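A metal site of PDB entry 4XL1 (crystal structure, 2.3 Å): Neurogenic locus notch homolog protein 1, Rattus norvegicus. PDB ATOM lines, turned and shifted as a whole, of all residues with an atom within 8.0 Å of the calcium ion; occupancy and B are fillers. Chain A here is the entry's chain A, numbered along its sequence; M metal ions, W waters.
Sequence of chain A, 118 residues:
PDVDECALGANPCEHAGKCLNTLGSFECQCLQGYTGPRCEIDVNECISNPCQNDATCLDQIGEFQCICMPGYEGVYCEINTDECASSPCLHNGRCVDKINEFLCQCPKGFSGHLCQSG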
ATOM      1  N   ASP A   4      16.956 -19.046 -10.265  1.00  0.00           N
ATOM      2  CA  ASP A   4      17.856 -19.053  -9.118  1.00  0.00           C
ATOM      3  C   ASP A   4      18.976 -20.067  -9.359  1.00  0.00           C
ATOM      4  O   ASP A   4      20.047 -19.709  -9.843  1.00  0.00           O
ATOM      5  CB  ASP A   4      17.079 -19.398  -7.844  1.00  0.00           C
ATOM      6  CG  ASP A   4      17.957 -19.419  -6.603  1.00  0.00           C
ATOM      7  OD1 ASP A   4      19.101 -18.929  -6.667  1.00  0.00           O
ATOM      8  OD2 ASP A   4      17.485 -19.930  -5.557  1.00  0.00           O
ATOM      9  N   GLU A   5      18.711 -21.324  -9.038  1.00  0.00           N
ATOM     10  CA  GLU A   5      19.727 -22.377  -9.098  1.00  0.00           C
ATOM     11  C   GLU A   5      19.975 -22.851 -10.520  1.00  0.00           C
ATOM     12  O   GLU A   5      21.060 -23.339 -10.841  1.00  0.00           O
ATOM     13  CB  GLU A   5      19.310 -23.549  -8.211  1.00  0.00           C
ATOM     14  CG  GLU A   5      20.450 -24.490  -7.866  1.00  0.00           C
ATOM     15  CD  GLU A   5      20.240 -25.204  -6.547  1.00  0.00           C
ATOM     16  OE1 GLU A   5      19.242 -24.890  -5.825  1.00  0.00           O
ATOM     17  OE2 GLU A   5      21.065 -26.087  -6.234  1.00  0.00           O
ATOM     18  N   CYS A   6      18.969 -22.714 -11.381  1.00  0.00           N
ATOM     19  CA  CYS A   6      19.108 -23.105 -12.776  1.00  0.00           C
ATOM     20  C   CYS A   6      20.093 -22.187 -13.495  1.00  0.00           C
ATOM     21  O   CYS A   6      20.656 -22.552 -14.526  1.00  0.00           O
ATOM     22  CB  CYS A   6      17.746 -23.066 -13.470  1.00  0.00           C
ATOM     23  SG  CYS A   6      16.476 -24.084 -12.680  1.00  0.00           S
ATOM     24  N   LEU A  20      13.438 -26.018 -13.051  1.00  0.00           N
ATOM     25  CA  LEU A  20      12.695 -25.107 -12.194  1.00  0.00           C
ATOM     26  C   LEU A  20      13.314 -25.053 -10.797  1.00  0.00           C
ATOM     27  O   LEU A  20      13.542 -26.100 -10.193  1.00  0.00           O
ATOM     28  CB  LEU A  20      11.228 -25.531 -12.086  1.00  0.00           C
ATOM     29  CG  LEU A  20      10.419 -25.665 -13.380  1.00  0.00           C
ATOM     30  CD1 LEU A  20       8.993 -26.080 -13.083  1.00  0.00           C
ATOM     31  CD2 LEU A  20      10.439 -24.344 -14.142  1.00  0.00           C
ATOM     32  N   ASN A  21      13.659 -23.871 -10.306  1.00  0.00           N
ATOM     33  CA  ASN A  21      14.243 -23.815  -8.962  1.00  0.00           C
ATOM     34  C   ASN A  21      13.190 -24.062  -7.907  1.00  0.00           C
ATOM     35  O   ASN A  21      12.053 -23.612  -8.000  1.00  0.00           O
ATOM     36  CB  ASN A  21      14.944 -22.480  -8.691  1.00  0.00           C
ATOM     37  CG  ASN A  21      15.332 -22.319  -7.209  1.00  0.00           C
ATOM     38  OD1 ASN A  21      16.195 -23.028  -6.681  1.00  0.00           O
ATOM     39  ND2 ASN A  21      14.687 -21.361  -6.541  1.00  0.00           N
ATOM     40  N   THR A  22      13.593 -24.786  -6.868  1.00  0.00           N
ATOM     41  CA  THR A  22      12.774 -24.997  -5.694  1.00  0.00           C
ATOM     42  C   THR A  22      13.604 -24.438  -4.581  1.00  0.00           C
ATOM     43  O   THR A  22      14.775 -24.129  -4.796  1.00  0.00           O
ATOM     44  CB  THR A  22      12.441 -26.463  -5.446  1.00  0.00           C
ATOM     45  OG1 THR A  22      13.661 -27.215  -5.376  1.00  0.00           O
ATOM     46  CG2 THR A  22      11.590 -27.019  -6.554  1.00  0.00           C
ATOM     47  N   LEU A  23      13.036 -24.310  -3.397  1.00  0.00           N
ATOM     48  CA  LEU A  23      13.788 -23.693  -2.322  1.00  0.00           C
ATOM     49  C   LEU A  23      14.964 -24.550  -1.882  1.00  0.00           C
ATOM     50  O   LEU A  23      14.809 -25.673  -1.426  1.00  0.00           O
ATOM     51  CB  LEU A  23      12.865 -23.368  -1.128  1.00  0.00           C
ATOM     52  CG  LEU A  23      13.587 -23.081   0.195  1.00  0.00           C
ATOM     53  CD1 LEU A  23      14.425 -21.839   0.104  1.00  0.00           C
ATOM     54  CD2 LEU A  23      12.498 -22.837   1.198  1.00  0.00           C
ATOM     55  N   GLY A  24      16.155 -24.009  -2.082  1.00  0.00           N
ATOM     56  CA  GLY A  24      17.347 -24.567  -1.474  1.00  0.00           C
ATOM     57  C   GLY A  24      17.843 -25.758  -2.265  1.00  0.00           C
ATOM     58  O   GLY A  24      18.683 -26.513  -1.803  1.00  0.00           O
ATOM     59  N   SER A  25      17.221 -25.976  -3.436  1.00  0.00           N
ATOM     60  CA  SER A  25      17.649 -26.989  -4.390  1.00  0.00           C
ATOM     61  C   SER A  25      16.911 -26.806  -5.731  1.00  0.00           C
ATOM     62  O   SER A  25      16.498 -25.678  -6.055  1.00  0.00           O
ATOM     63  CB  SER A  25      17.429 -28.417  -3.888  1.00  0.00           C
ATOM     64  OG  SER A  25      18.074 -29.177  -4.874  1.00  0.00           O
ATOM     65  N   PHE A  26      16.724 -27.897  -6.511  1.00  0.00           N
ATOM     66  CA  PHE A  26      15.980 -27.796  -7.780  1.00  0.00           C
ATOM     67  C   PHE A  26      15.279 -29.063  -8.338  1.00  0.00           C
ATOM     68  O   PHE A  26      15.527 -30.179  -7.856  1.00  0.00           O
ATOM     69  CB  PHE A  26      16.898 -27.240  -8.882  1.00  0.00           C
ATOM     70  CG  PHE A  26      17.723 -28.283  -9.607  1.00  0.00           C
ATOM     71  CD1 PHE A  26      18.953 -28.713  -9.129  1.00  0.00           C
ATOM     72  CD2 PHE A  26      17.282 -28.792 -10.825  1.00  0.00           C
ATOM     73  CE1 PHE A  26      19.707 -29.647  -9.844  1.00  0.00           C
ATOM     74  CE2 PHE A  26      18.029 -29.736 -11.524  1.00  0.00           C
ATOM     75  CZ  PHE A  26      19.240 -30.154 -11.035  1.00  0.00           C
ATOM     76  N   GLU A  27      14.421 -28.882  -9.356  1.00  0.00           N
ATOM     77  CA  GLU A  27      13.788 -30.017 -10.079  1.00  0.00           C
ATOM     78  C   GLU A  27      13.571 -29.841 -11.614  1.00  0.00           C
ATOM     79  O   GLU A  27      13.497 -28.733 -12.148  1.00  0.00           O
ATOM     80  CB  GLU A  27      12.422 -30.367  -9.473  1.00  0.00           C
ATOM     81  CG  GLU A  27      11.310 -29.362  -9.728  1.00  0.00           C
ATOM     82  CD  GLU A  27      10.133 -29.555  -8.785  1.00  0.00           C
ATOM     83  OE1 GLU A  27      10.110 -30.568  -8.060  1.00  0.00           O
ATOM     84  OE2 GLU A  27       9.221 -28.700  -8.788  1.00  0.00           O
HETATM   85 CA    CA M   1      16.992 -23.860  -4.173  1.00  0.00          CA
HETATM   86  O   HOH W   1      16.447 -21.523  -3.270  1.00  0.00           O
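O of Ser 25 lies close to OG1 of Thr 22. OG1 of Thr 22 lies within hydrogen-bond range of N of Phe 26 (3.3 Å). The side-chain amide nitrogen (ND2) of Asn 21 sits at hydrogen-bond distance from the side-chain carboxylate (OD2) of Asp 4, at 3.3 Å. The side-chain carboxylate of Glu 5 sits close to the backbone NH of Ser 25, 3.3 Å away. SG of Cys 6 lies within hydrogen-bond range of N of Asn 21 (3.7 Å).
C of Leu 23 touches the calcium ion, 3.1 Å away. Within 4 Å of the calcium ion: Glu 5, Asn 21, Thr 22, Leu 23, Gly 24 and Ser 25. Along chain A the residues within 4 Å of the calcium ion span positions 5 to 25. The nearest printed residue that does not touch the calcium ion is Asp 4 (4.2 Å).
The calcium ion is bound by N of Ser 25 (2.3 Å), N of Gly 24 (2.3 Å), O of Thr 22 (2.3 Å), water W1 (2.6 Å), O of Ser 25 (2.7 Å) and OD1 of Asn 21 (2.8 Å). Slightly farther from the calcium ion lies the side-chain carboxylate (OE1) of Glu 5 (3.0 Å).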
